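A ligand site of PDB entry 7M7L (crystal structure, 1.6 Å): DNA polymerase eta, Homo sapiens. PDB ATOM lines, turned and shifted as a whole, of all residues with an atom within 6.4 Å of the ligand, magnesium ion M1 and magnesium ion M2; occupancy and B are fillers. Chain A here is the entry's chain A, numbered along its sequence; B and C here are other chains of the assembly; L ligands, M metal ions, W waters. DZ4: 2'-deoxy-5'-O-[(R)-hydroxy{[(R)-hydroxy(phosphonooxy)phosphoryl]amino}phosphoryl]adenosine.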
ATOM      1  N   ASP A  16     -11.692  10.927   5.160  1.00  0.00           N
ATOM      2  CA  ASP A  16     -10.420  11.391   5.714  1.00  0.00           C
ATOM      3  C   ASP A  16      -9.258  10.657   5.066  1.00  0.00           C
ATOM      4  O   ASP A  16      -9.196   9.420   5.083  1.00  0.00           O
ATOM      5  CB  ASP A  16     -10.372  11.184   7.237  1.00  0.00           C
ATOM      6  CG  ASP A  16      -9.113  11.740   7.852  1.00  0.00           C
ATOM      7  OD1 ASP A  16      -8.070  11.077   7.748  1.00  0.00           O
ATOM      8  OD2 ASP A  16      -9.154  12.852   8.387  1.00  0.00           O
ATOM      9  N   MET A  17      -8.301  11.423   4.558  1.00  0.00           N
ATOM     10  CA  MET A  17      -7.163  10.827   3.858  1.00  0.00           C
ATOM     11  C   MET A  17      -6.287  10.012   4.817  1.00  0.00           C
ATOM     12  O   MET A  17      -6.103  10.367   5.976  1.00  0.00           O
ATOM     13  CB  MET A  17      -6.334  11.933   3.196  1.00  0.00           C
ATOM     14  CG  MET A  17      -7.122  12.829   2.250  1.00  0.00           C
ATOM     15  SD  MET A  17      -8.111  11.982   0.992  1.00  0.00           S
ATOM     16  CE  MET A  17      -6.883  11.181   0.040  1.00  0.00           C
ATOM     17  N   ASP A  18      -5.769   8.884   4.315  1.00  0.00           N
ATOM     18  CA  ASP A  18      -4.845   8.072   5.115  1.00  0.00           C
ATOM     19  C   ASP A  18      -3.464   8.706   5.071  1.00  0.00           C
ATOM     20  O   ASP A  18      -3.003   9.147   4.018  1.00  0.00           O
ATOM     21  CB  ASP A  18      -4.800   6.646   4.576  1.00  0.00           C
ATOM     22  CG  ASP A  18      -6.166   5.936   4.626  1.00  0.00           C
ATOM     23  OD1 ASP A  18      -7.012   6.281   5.484  1.00  0.00           O
ATOM     24  OD2 ASP A  18      -6.381   5.024   3.829  1.00  0.00           O
ATOM     25  N   CYS A  19      -2.826   8.776   6.247  1.00  0.00           N
ATOM     26  CA  CYS A  19      -1.502   9.388   6.453  1.00  0.00           C
ATOM     27  C   CYS A  19      -1.202  10.432   5.393  1.00  0.00           C
ATOM     28  O   CYS A  19      -0.281  10.280   4.577  1.00  0.00           O
ATOM     29  CB  CYS A  19      -0.403   8.310   6.533  1.00  0.00           C
ATOM     30  SG  CYS A  19      -0.277   7.104   5.184  1.00  0.00           S
ATOM     31  N   PHE A  20      -1.991  11.505   5.381  1.00  0.00           N
ATOM     32  CA  PHE A  20      -2.115  12.333   4.177  1.00  0.00           C
ATOM     33  C   PHE A  20      -0.786  12.889   3.681  1.00  0.00           C
ATOM     34  O   PHE A  20      -0.441  12.720   2.505  1.00  0.00           O
ATOM     35  CB  PHE A  20      -3.107  13.453   4.412  1.00  0.00           C
ATOM     36  CG  PHE A  20      -3.360  14.287   3.206  1.00  0.00           C
ATOM     37  CD1 PHE A  20      -3.553  13.705   1.960  1.00  0.00           C
ATOM     38  CD2 PHE A  20      -3.416  15.660   3.316  1.00  0.00           C
ATOM     39  CE1 PHE A  20      -3.805  14.482   0.829  1.00  0.00           C
ATOM     40  CE2 PHE A  20      -3.665  16.450   2.180  1.00  0.00           C
ATOM     41  CZ  PHE A  20      -3.861  15.852   0.953  1.00  0.00           C
ATOM     42  N   PHE A  21      -0.052  13.633   4.530  1.00  0.00           N
ATOM     43  CA  PHE A  21       1.170  14.274   4.032  1.00  0.00           C
ATOM     44  C   PHE A  21       2.179  13.234   3.559  1.00  0.00           C
ATOM     45  O   PHE A  21       2.917  13.465   2.601  1.00  0.00           O
ATOM     46  CB  PHE A  21       1.817  15.167   5.086  1.00  0.00           C
ATOM     47  CG  PHE A  21       1.050  16.443   5.416  1.00  0.00           C
ATOM     48  CD1 PHE A  21      -0.259  16.646   5.007  1.00  0.00           C
ATOM     49  CD2 PHE A  21       1.671  17.431   6.150  1.00  0.00           C
ATOM     50  CE1 PHE A  21      -0.933  17.822   5.337  1.00  0.00           C
ATOM     51  CE2 PHE A  21       1.003  18.613   6.481  1.00  0.00           C
ATOM     52  CZ  PHE A  21      -0.296  18.807   6.070  1.00  0.00           C
ATOM     53  N   VAL A  22       2.204  12.066   4.218  1.00  0.00           N
ATOM     54  CA  VAL A  22       3.064  10.979   3.756  1.00  0.00           C
ATOM     55  C   VAL A  22       2.663  10.542   2.350  1.00  0.00           C
ATOM     56  O   VAL A  22       3.513  10.341   1.491  1.00  0.00           O
ATOM     57  CB  VAL A  22       3.027   9.796   4.745  1.00  0.00           C
ATOM     58  CG1 VAL A  22       3.641   8.543   4.107  1.00  0.00           C
ATOM     59  CG2 VAL A  22       3.757  10.150   6.030  1.00  0.00           C
ATOM     60  N   GLN A  41       9.065  18.401  10.002  1.00  0.00           N
ATOM     61  CA  GLN A  41       9.259  19.866   9.892  1.00  0.00           C
ATOM     62  C   GLN A  41      10.505  20.262  10.671  1.00  0.00           C
ATOM     63  O   GLN A  41      10.600  19.918  11.812  1.00  0.00           O
ATOM     64  CB  GLN A  41       8.130  20.739  10.458  1.00  0.00           C
ATOM     65  CG  GLN A  41       6.724  20.382  10.051  1.00  0.00           C
ATOM     66  CD  GLN A  41       5.813  21.455  10.577  1.00  0.00           C
ATOM     67  OE1 GLN A  41       5.279  22.255   9.820  1.00  0.00           O
ATOM     68  NE2 GLN A  41       5.667  21.505  11.896  1.00  0.00           N
ATOM     69  N   ILE A  51       5.148  15.190  11.715  1.00  0.00           N
ATOM     70  CA  ILE A  51       3.753  15.598  11.623  1.00  0.00           C
ATOM     71  C   ILE A  51       2.864  14.586  10.907  1.00  0.00           C
ATOM     72  O   ILE A  51       1.635  14.732  10.967  1.00  0.00           O
ATOM     73  CB  ILE A  51       3.603  17.002  10.971  1.00  0.00           C
ATOM     74  CG1 ILE A  51       4.207  17.035   9.567  1.00  0.00           C
ATOM     75  CG2 ILE A  51       4.247  18.058  11.862  1.00  0.00           C
ATOM     76  CD1 ILE A  51       3.875  18.354   8.825  1.00  0.00           C
ATOM     77  N   ALA A  52       3.427  13.552  10.262  1.00  0.00           N
ATOM     78  CA  ALA A  52       2.627  12.523   9.605  1.00  0.00           C
ATOM     79  C   ALA A  52       3.457  11.245   9.510  1.00  0.00           C
ATOM     80  O   ALA A  52       4.680  11.315   9.348  1.00  0.00           O
ATOM     81  CB  ALA A  52       2.176  12.953   8.197  1.00  0.00           C
ATOM     82  N   VAL A  53       2.798  10.089   9.623  1.00  0.00           N
ATOM     83  CA  VAL A  53       3.482   8.806   9.806  1.00  0.00           C
ATOM     84  C   VAL A  53       2.791   7.733   8.971  1.00  0.00           C
ATOM     85  O   VAL A  53       1.576   7.525   9.113  1.00  0.00           O
ATOM     86  CB  VAL A  53       3.477   8.367  11.292  1.00  0.00           C
ATOM     87  CG1 VAL A  53       4.362   7.147  11.488  1.00  0.00           C
ATOM     88  CG2 VAL A  53       3.939   9.483  12.201  1.00  0.00           C
ATOM     89  N   TYR A  55       1.644   3.930   7.843  1.00  0.00           N
ATOM     90  CA  TYR A  55       1.154   2.856   8.709  1.00  0.00           C
ATOM     91  C   TYR A  55       2.255   1.831   9.001  1.00  0.00           C
ATOM     92  O   TYR A  55       2.333   1.289  10.110  1.00  0.00           O
ATOM     93  CB  TYR A  55      -0.092   2.210   8.104  1.00  0.00           C
ATOM     94  CG  TYR A  55      -1.310   3.064   8.381  1.00  0.00           C
ATOM     95  CD1 TYR A  55      -1.597   4.180   7.584  1.00  0.00           C
ATOM     96  CD2 TYR A  55      -2.124   2.819   9.476  1.00  0.00           C
ATOM     97  CE1 TYR A  55      -2.686   4.997   7.864  1.00  0.00           C
ATOM     98  CE2 TYR A  55      -3.216   3.623   9.761  1.00  0.00           C
ATOM     99  CZ  TYR A  55      -3.491   4.712   8.959  1.00  0.00           C
ATOM    100  OH  TYR A  55      -4.565   5.513   9.242  1.00  0.00           O
ATOM    101  N   ARG A  58       4.008   3.377  11.840  1.00  0.00           N
ATOM    102  CA  ARG A  58       3.219   3.305  13.069  1.00  0.00           C
ATOM    103  C   ARG A  58       3.370   1.955  13.746  1.00  0.00           C
ATOM    104  O   ARG A  58       3.309   1.868  14.977  1.00  0.00           O
ATOM    105  CB  ARG A  58       1.741   3.570  12.771  1.00  0.00           C
ATOM    106  CG  ARG A  58       1.482   4.930  12.201  1.00  0.00           C
ATOM    107  CD  ARG A  58       0.013   5.158  11.975  1.00  0.00           C
ATOM    108  NE  ARG A  58      -0.156   6.308  11.094  1.00  0.00           N
ATOM    109  CZ  ARG A  58      -1.296   6.949  10.880  1.00  0.00           C
ATOM    110  NH1 ARG A  58      -2.408   6.554  11.502  1.00  0.00           N
ATOM    111  NH2 ARG A  58      -1.319   7.981  10.037  1.00  0.00           N
ATOM    112  N   ARG A  64       2.990  11.048  15.454  1.00  0.00           N
ATOM    113  CA  ARG A  64       3.021  12.497  15.331  1.00  0.00           C
ATOM    114  C   ARG A  64       3.510  13.120  16.641  1.00  0.00           C
ATOM    115  O   ARG A  64       3.272  12.595  17.735  1.00  0.00           O
ATOM    116  CB  ARG A  64       1.608  12.994  14.990  1.00  0.00           C
ATOM    117  CG  ARG A  64       1.413  14.492  14.877  1.00  0.00           C
ATOM    118  CD  ARG A  64      -0.042  14.763  14.479  1.00  0.00           C
ATOM    119  NE  ARG A  64      -0.954  13.960  15.289  1.00  0.00           N
ATOM    120  CZ  ARG A  64      -2.135  13.494  14.875  1.00  0.00           C
ATOM    121  NH1 ARG A  64      -2.574  13.735  13.646  1.00  0.00           N
ATOM    122  NH2 ARG A  64      -2.880  12.760  15.700  1.00  0.00           N
ATOM    123  N   LEU A  92       3.380  24.982   3.809  1.00  0.00           N
ATOM    124  CA  LEU A  92       2.496  23.834   3.629  1.00  0.00           C
ATOM    125  C   LEU A  92       1.794  23.831   2.274  1.00  0.00           C
ATOM    126  O   LEU A  92       0.835  23.062   2.076  1.00  0.00           O
ATOM    127  CB  LEU A  92       1.478  23.800   4.772  1.00  0.00           C
ATOM    128  CG  LEU A  92       2.097  23.781   6.175  1.00  0.00           C
ATOM    129  CD1 LEU A  92       1.006  23.826   7.228  1.00  0.00           C
ATOM    130  CD2 LEU A  92       2.940  22.539   6.332  1.00  0.00           C
ATOM    131  N   SER A 116     -10.964  19.788   7.423  1.00  0.00           N
ATOM    132  CA  SER A 116      -9.544  19.956   7.713  1.00  0.00           C
ATOM    133  C   SER A 116      -8.814  19.946   6.376  1.00  0.00           C
ATOM    134  O   SER A 116      -9.426  19.814   5.317  1.00  0.00           O
ATOM    135  CB  SER A 116      -9.013  18.865   8.651  1.00  0.00           C
ATOM    136  OG  SER A 116      -8.784  17.652   7.947  1.00  0.00           O
ATOM    137  N   ILE A 117      -7.485  20.027   6.443  1.00  0.00           N
ATOM    138  CA  ILE A 117      -6.727  19.911   5.207  1.00  0.00           C
ATOM    139  C   ILE A 117      -6.943  18.551   4.539  1.00  0.00           C
ATOM    140  O   ILE A 117      -6.776  18.417   3.332  1.00  0.00           O
ATOM    141  CB  ILE A 117      -5.225  20.175   5.463  1.00  0.00           C
ATOM    142  CG1 ILE A 117      -4.520  20.543   4.150  1.00  0.00           C
ATOM    143  CG2 ILE A 117      -4.576  18.974   6.109  1.00  0.00           C
ATOM    144  CD1 ILE A 117      -3.094  21.075   4.352  1.00  0.00           C
ATOM    145  N   ASP A 118      -7.337  17.523   5.302  1.00  0.00           N
ATOM    146  CA  ASP A 118      -7.400  16.194   4.707  1.00  0.00           C
ATOM    147  C   ASP A 118      -8.763  15.520   4.879  1.00  0.00           C
ATOM    148  O   ASP A 118      -8.869  14.294   4.659  1.00  0.00           O
ATOM    149  CB  ASP A 118      -6.290  15.284   5.237  1.00  0.00           C
ATOM    150  CG  ASP A 118      -6.710  14.449   6.443  1.00  0.00           C
ATOM    151  OD1 ASP A 118      -7.360  14.982   7.389  1.00  0.00           O
ATOM    152  OD2 ASP A 118      -6.373  13.246   6.429  1.00  0.00           O
ATOM    153  N   GLU A 119      -9.811  16.251   5.235  1.00  0.00           N
ATOM    154  CA  GLU A 119     -11.102  15.592   5.379  1.00  0.00           C
ATOM    155  C   GLU A 119     -12.257  16.538   5.117  1.00  0.00           C
ATOM    156  O   GLU A 119     -12.163  17.760   5.344  1.00  0.00           O
ATOM    157  CB  GLU A 119     -11.286  14.964   6.761  1.00  0.00           C
ATOM    158  CG  GLU A 119     -11.469  15.956   7.890  1.00  0.00           C
ATOM    159  CD  GLU A 119     -10.857  15.433   9.160  1.00  0.00           C
ATOM    160  OE1 GLU A 119     -11.605  14.945  10.033  1.00  0.00           O
ATOM    161  OE2 GLU A 119      -9.619  15.483   9.288  1.00  0.00           O
ATOM    162  N   SER A 216     -10.016   6.794   4.015  1.00  0.00           N
ATOM    163  CA  SER A 216     -11.049   6.052   4.703  1.00  0.00           C
ATOM    164  C   SER A 216     -12.294   6.917   4.811  1.00  0.00           C
ATOM    165  O   SER A 216     -12.257   8.119   4.531  1.00  0.00           O
ATOM    166  CB  SER A 216     -10.579   5.604   6.093  1.00  0.00           C
ATOM    167  OG  SER A 216      -9.447   4.747   5.955  1.00  0.00           O
ATOM    168  N   LYS A 234      -9.676   2.389   9.576  1.00  0.00           N
ATOM    169  CA  LYS A 234      -8.518   2.924   8.879  1.00  0.00           C
ATOM    170  C   LYS A 234      -7.353   1.934   8.895  1.00  0.00           C
ATOM    171  O   LYS A 234      -7.137   1.258   9.909  1.00  0.00           O
ATOM    172  CB  LYS A 234      -8.071   4.231   9.530  1.00  0.00           C
ATOM    173  CG  LYS A 234      -8.466   5.467   8.803  1.00  0.00           C
ATOM    174  CD  LYS A 234      -7.924   6.715   9.461  1.00  0.00           C
ATOM    175  CE  LYS A 234      -8.373   7.956   8.700  1.00  0.00           C
ATOM    176  NZ  LYS A 234      -7.603   8.186   7.437  1.00  0.00           N
ATOM    177  N   PRO A 235      -6.559   1.856   7.823  1.00  0.00           N
ATOM    178  CA  PRO A 235      -6.646   2.664   6.600  1.00  0.00           C
ATOM    179  C   PRO A 235      -7.349   1.950   5.445  1.00  0.00           C
ATOM    180  O   PRO A 235      -7.567   0.740   5.512  1.00  0.00           O
ATOM    181  CB  PRO A 235      -5.190   2.913   6.241  1.00  0.00           C
ATOM    182  CG  PRO A 235      -4.534   1.597   6.635  1.00  0.00           C
ATOM    183  CD  PRO A 235      -5.305   1.080   7.842  1.00  0.00           C
ATOM    184  P    DA B   8      -9.131  15.821  15.349  1.00  0.00           P
ATOM    185  OP1  DA B   8      -9.793  14.584  14.878  1.00  0.00           O
ATOM    186  OP2  DA B   8      -7.871  15.686  16.119  1.00  0.00           O
ATOM    187  O5'  DA B   8      -8.957  16.907  14.135  1.00  0.00           O
ATOM    188  C5'  DA B   8      -9.393  16.744  12.734  1.00  0.00           C
ATOM    189  C4'  DA B   8      -8.203  17.193  11.896  1.00  0.00           C
ATOM    190  O4'  DA B   8      -7.514  18.300  12.529  1.00  0.00           O
ATOM    191  C3'  DA B   8      -7.162  16.110  11.660  1.00  0.00           C
ATOM    192  O3'  DA B   8      -6.999  15.880  10.248  1.00  0.00           O
ATOM    193  C2'  DA B   8      -5.877  16.629  12.332  1.00  0.00           C
ATOM    194  C1'  DA B   8      -6.117  18.130  12.416  1.00  0.00           C
ATOM    195  N9   DA B   8      -5.486  18.741  13.588  1.00  0.00           N
ATOM    196  C8   DA B   8      -5.718  18.440  14.906  1.00  0.00           C
ATOM    197  N7   DA B   8      -5.013  19.157  15.751  1.00  0.00           N
ATOM    198  C5   DA B   8      -4.266  19.991  14.931  1.00  0.00           C
ATOM    199  C6   DA B   8      -3.305  20.983  15.202  1.00  0.00           C
ATOM    200  N6   DA B   8      -2.939  21.336  16.440  1.00  0.00           N
ATOM    201  N1   DA B   8      -2.753  21.620  14.162  1.00  0.00           N
ATOM    202  C2   DA B   8      -3.120  21.267  12.923  1.00  0.00           C
ATOM    203  N3   DA B   8      -4.006  20.360  12.544  1.00  0.00           N
ATOM    204  C4   DA B   8      -4.549  19.741  13.594  1.00  0.00           C
ATOM    205  P    DT C   3       8.570  20.053  23.600  1.00  0.00           P
ATOM    206  OP1  DT C   3       8.134  20.659  24.871  1.00  0.00           O
ATOM    207  OP2  DT C   3       9.082  18.666  23.559  1.00  0.00           O
ATOM    208  O5'  DT C   3       7.363  20.131  22.551  1.00  0.00           O
ATOM    209  C5'  DT C   3       7.311  19.223  21.461  1.00  0.00           C
ATOM    210  C4'  DT C   3       6.808  19.907  20.205  1.00  0.00           C
ATOM    211  O4'  DT C   3       5.674  19.172  19.680  1.00  0.00           O
ATOM    212  C3'  DT C   3       6.285  21.322  20.425  1.00  0.00           C
ATOM    213  O3'  DT C   3       6.349  22.051  19.224  1.00  0.00           O
ATOM    214  C2'  DT C   3       4.838  21.069  20.840  1.00  0.00           C
ATOM    215  C1'  DT C   3       4.464  19.825  20.040  1.00  0.00           C
ATOM    216  N1   DT C   3       3.631  18.869  20.818  1.00  0.00           N
ATOM    217  C2   DT C   3       2.581  18.237  20.195  1.00  0.00           C
ATOM    218  O2   DT C   3       2.287  18.415  19.028  1.00  0.00           O
ATOM    219  N3   DT C   3       1.870  17.379  21.009  1.00  0.00           N
ATOM    220  C4   DT C   3       2.121  17.101  22.345  1.00  0.00           C
ATOM    221  O4   DT C   3       1.424  16.316  22.986  1.00  0.00           O
ATOM    222  C5   DT C   3       3.240  17.798  22.928  1.00  0.00           C
ATOM    223  C7   DT C   3       3.594  17.586  24.368  1.00  0.00           C
ATOM    224  C6   DT C   3       3.933  18.641  22.147  1.00  0.00           C
ATOM    225  P    DT C   4       6.839  23.576  19.231  1.00  0.00           P
ATOM    226  OP1  DT C   4       8.259  23.612  19.618  1.00  0.00           O
ATOM    227  OP2  DT C   4       5.823  24.361  19.964  1.00  0.00           O
ATOM    228  O5'  DT C   4       6.722  24.006  17.704  1.00  0.00           O
ATOM    229  C5'  DT C   4       7.437  23.305  16.723  1.00  0.00           C
ATOM    230  C4'  DT C   4       6.771  23.513  15.379  1.00  0.00           C
ATOM    231  O4'  DT C   4       5.660  22.603  15.245  1.00  0.00           O
ATOM    232  C3'  DT C   4       6.212  24.907  15.142  1.00  0.00           C
ATOM    233  O3'  DT C   4       6.475  25.251  13.810  1.00  0.00           O
ATOM    234  C2'  DT C   4       4.701  24.719  15.392  1.00  0.00           C
ATOM    235  C1'  DT C   4       4.497  23.306  14.878  1.00  0.00           C
ATOM    236  N1   DT C   4       3.340  22.596  15.469  1.00  0.00           N
ATOM    237  C2   DT C   4       2.560  21.856  14.629  1.00  0.00           C
ATOM    238  O2   DT C   4       2.758  21.789  13.435  1.00  0.00           O
ATOM    239  N3   DT C   4       1.526  21.200  15.241  1.00  0.00           N
ATOM    240  C4   DT C   4       1.218  21.199  16.577  1.00  0.00           C
ATOM    241  O4   DT C   4       0.264  20.560  17.016  1.00  0.00           O
ATOM    242  C5   DT C   4       2.085  21.994  17.417  1.00  0.00           C
ATOM    243  C7   DT C   4       1.845  22.074  18.903  1.00  0.00           C
ATOM    244  C6   DT C   4       3.107  22.643  16.826  1.00  0.00           C
ATOM    245  P    DT C   5       6.006  26.663  13.220  1.00  0.00           P
ATOM    246  OP1  DT C   5       7.042  27.065  12.242  1.00  0.00           O
ATOM    247  OP2  DT C   5       5.641  27.573  14.331  1.00  0.00           O
ATOM    248  O5'  DT C   5       4.659  26.313  12.460  1.00  0.00           O
ATOM    249  C5'  DT C   5       4.705  25.554  11.259  1.00  0.00           C
ATOM    250  C4'  DT C   5       3.310  25.433  10.689  1.00  0.00           C
ATOM    251  O4'  DT C   5       2.484  24.655  11.587  1.00  0.00           O
ATOM    252  C3'  DT C   5       2.594  26.768  10.488  1.00  0.00           C
ATOM    253  O3'  DT C   5       1.943  26.756   9.217  1.00  0.00           O
ATOM    254  C2'  DT C   5       1.584  26.798  11.643  1.00  0.00           C
ATOM    255  C1'  DT C   5       1.256  25.316  11.748  1.00  0.00           C
ATOM    256  N1   DT C   5       0.667  24.891  13.017  1.00  0.00           N
ATOM    257  C2   DT C   5      -0.286  23.910  12.993  1.00  0.00           C
ATOM    258  O2   DT C   5      -0.665  23.387  11.974  1.00  0.00           O
ATOM    259  N3   DT C   5      -0.775  23.559  14.224  1.00  0.00           N
ATOM    260  C4   DT C   5      -0.414  24.068  15.450  1.00  0.00           C
ATOM    261  O4   DT C   5      -0.928  23.686  16.495  1.00  0.00           O
ATOM    262  C5   DT C   5       0.597  25.100  15.409  1.00  0.00           C
ATOM    263  C7   DT C   5       1.073  25.728  16.684  1.00  0.00           C
ATOM    264  C6   DT C   5       1.090  25.455  14.216  1.00  0.00           C
HETATM  265  N1  DZ4 L   1       0.120  19.654  13.493  1.00  0.00           N
HETATM  266  C2  DZ4 L   1       0.409  19.816  12.197  1.00  0.00           C
HETATM  267  N3  DZ4 L   1      -0.055  19.138  11.150  1.00  0.00           N
HETATM  268  C4  DZ4 L   1      -0.902  18.184  11.546  1.00  0.00           C
HETATM  269  C5  DZ4 L   1      -1.293  17.896  12.829  1.00  0.00           C
HETATM  270  C6  DZ4 L   1      -0.746  18.681  13.851  1.00  0.00           C
HETATM  271  N6  DZ4 L   1      -1.055  18.484  15.127  1.00  0.00           N
HETATM  272  N7  DZ4 L   1      -2.194  16.840  12.833  1.00  0.00           N
HETATM  273  C8  DZ4 L   1      -2.321  16.515  11.570  1.00  0.00           C
HETATM  274  N9  DZ4 L   1      -1.562  17.292  10.745  1.00  0.00           N
HETATM  275  PA  DZ4 L   1      -4.838  13.400  10.187  1.00  0.00           P
HETATM  276  PB  DZ4 L   1      -3.217  11.461   8.814  1.00  0.00           P
HETATM  277  PG  DZ4 L   1      -4.699   9.068   9.354  1.00  0.00           P
HETATM  278  C1' DZ4 L   1      -1.449  17.213   9.285  1.00  0.00           C
HETATM  279  O1A DZ4 L   1      -6.039  13.131   9.423  1.00  0.00           O
HETATM  280  O1B DZ4 L   1      -3.967  11.768   7.600  1.00  0.00           O
HETATM  281  O1G DZ4 L   1      -5.799  10.003   9.066  1.00  0.00           O
HETATM  282  C2' DZ4 L   1      -0.532  16.098   8.794  1.00  0.00           C
HETATM  283  O2A DZ4 L   1      -5.161  13.627  11.682  1.00  0.00           O
HETATM  284  O2B DZ4 L   1      -1.703  11.714   8.598  1.00  0.00           O
HETATM  285  O2G DZ4 L   1      -4.610   7.963   8.372  1.00  0.00           O
HETATM  286  C3' DZ4 L   1      -1.515  14.976   8.470  1.00  0.00           C
HETATM  287  O3' DZ4 L   1      -1.036  14.105   7.456  1.00  0.00           O
HETATM  288  N3A DZ4 L   1      -3.716  12.246  10.128  1.00  0.00           N
HETATM  289  O3B DZ4 L   1      -3.357   9.915   9.166  1.00  0.00           O
HETATM  290  O3G DZ4 L   1      -4.696   8.600  10.784  1.00  0.00           O
HETATM  291  C4' DZ4 L   1      -2.744  15.738   8.002  1.00  0.00           C
HETATM  292  O4' DZ4 L   1      -2.741  16.976   8.740  1.00  0.00           O
HETATM  293  C5' DZ4 L   1      -4.048  15.031   8.259  1.00  0.00           C
HETATM  294  O5' DZ4 L   1      -4.200  14.778   9.663  1.00  0.00           O
HETATM  295 MG    MG M   1      -6.111  11.599   7.664  1.00  0.00          MG
HETATM  296 MG    MG M   2      -7.941  14.224   9.199  1.00  0.00          MG
HETATM  297  O   HOH W   1      -5.446  17.795   9.259  1.00  0.00           O
HETATM  298  O   HOH W   2       0.549  20.817   8.971  1.00  0.00           O
HETATM  299  O   HOH W   3      -8.284  13.274  11.072  1.00  0.00           O
HETATM  300  O   HOH W   4      -3.411  20.074   9.781  1.00  0.00           O
HETATM  301  O   HOH W   5      -6.424  12.979  13.881  1.00  0.00           O
HETATM  302  O   HOH W   6      -3.469  10.049  12.684  1.00  0.00           O
HETATM  303  O   HOH W   7      -0.906  13.290  11.582  1.00  0.00           O
HETATM  304  O   HOH W   8      -7.781  10.505  11.036  1.00  0.00           O
HETATM  305  O   HOH W   9      -3.140  16.303  15.720  1.00  0.00           O
HETATM  306  O   HOH W  10       0.085  10.479  10.197  1.00  0.00           O
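The side-chain hydroxyl of Tyr 55 lies within hydrogen-bond range of an oxygen (O2G) of the ligand, at 2.6 Å. A nitrogen (N6) of the ligand lies within hydrogen-bond range of O4 of DT 4 of chain C. N of Cys 19 sits at hydrogen-bond distance from O2G of the ligand, 2.9 Å away. The guanidinium group (NH1) of Arg 58 lies within salt-bridge range of an oxygen (O3G) of the ligand, at 3.2 Å. The backbone NH (N) of Phe 20 sits at hydrogen-bond distance from an oxygen (O2B) of the ligand, at 3.2 Å. O2G of the ligand is in salt-bridge range of NZ of Lys 234 (3.1 Å). O3' of the ligand lies within hydrogen-bond range of N of Phe 21, at 3.1 Å. O2A of the ligand lies within salt-bridge range of NH1 of Arg 64, at 3.2 Å.
O of Ser 216 lies within hydrogen-bond range of N of Asp 16. The backbone NH (N) of Asp 118 sits at hydrogen-bond distance from the side-chain hydroxyl (OG) of Ser 116 (3.0 Å). NZ of Lys 234 lies close to O of Met 17, at 3.0 Å. The side-chain hydroxyl of Ser 116 lies close to the backbone NH of Glu 119, 3.2 Å away. O3' of DA 8 of chain B sits close to the side-chain hydroxyl (OG) of Ser 116, at 3.4 Å. NE2 of Gln 41 lies within hydrogen-bond range of O2 of DT 4 of chain C, 3.3 Å away. The side-chain amino group of Lys 234 lies within salt-bridge range of the side-chain carboxylate of Asp 18 (2.8 Å). The side-chain carboxylate (OD1) of Asp 18 is in hydrogen-bond range of the side-chain hydroxyl (OG) of Ser 216, at 2.9 Å.
Asp 18 touches the ligand (CA to O2G, 3.3 Å). Ile 51 touches the ligand (O to C2', 3.4 Å). Ala 52 touches the ligand (CB to O3', 3.5 Å). Ile 117 touches the ligand. DT 5 of chain C touches the ligand. Hydrophobic or aromatic side chains that line the ligand: Phe 20, Phe 21, Ala 52, Tyr 55 and Ile 117. 17 residues have an atom within 4 Å of the ligand: Asp 16, Met 17, Asp 18, Cys 19, Phe 20, Phe 21, Ile 51, Ala 52, Tyr 55, Arg 58, Arg 64, Ile 117, Asp 118, Lys 234, DA 8 of chain B, DT 4 of chain C and DT 5 of chain C.
NZ of Lys 234 touches magnesium ion M1, at 3.7 Å. Four residues have an atom within 4 Å of magnesium ion M1: Asp 16, Met 17, Asp 118 and Lys 234. The nearest printed residue that does not touch magnesium ion M1 is Asp 18 (4.3 Å).
Residues that only touch magnesium ion M2: Ser 116.
OD1 of Asp 16 binds magnesium ion M1, at 2.0 Å. OD2 of Asp 118 is bound to magnesium ion M1 (2.1 Å). O of Met 17 is bound to magnesium ion M1. Magnesium ion M1 is bound by O1G of the ligand (2.1 Å). An oxygen (O1B) of the ligand binds magnesium ion M1 (2.2 Å). O1A of the ligand is bound to magnesium ion M1, at 2.3 Å. Magnesium ion M1 has six donor atoms within binding distance.
Magnesium ion M2 is bound by the side-chain carboxylate of Asp 16 (2.0 Å), the side-chain carboxylate of Asp 118 (2.0 Å), the side-chain carboxylate of Glu 119 (2.1 Å), water W3 (2.1 Å), O3' of DA 8 of chain B (2.2 Å) and an oxygen (O1A) of the ligand (2.2 Å). Magnesium ion M2 has six donor atoms within binding distance.
Water W10 lies within hydrogen-bond range of O2B of the ligand, N of Val 53 and NH2 of Arg 58. Water W9 lies within hydrogen-bond range of N6 of the ligand (3.1 Å), NE of Arg 64 (3.2 Å) and N7 of DA 8 of chain B (3.4 Å). Water W7 lies within hydrogen-bond range of the guanidinium group of Arg 64, the backbone carbonyl oxygen of Ile 51 and a nitrogen (N3A) of the ligand. Water W4 lies within hydrogen-bond range of N3 of DA 8 of chain B (2.8 Å) and an oxygen (O4') of the ligand (3.3 Å).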
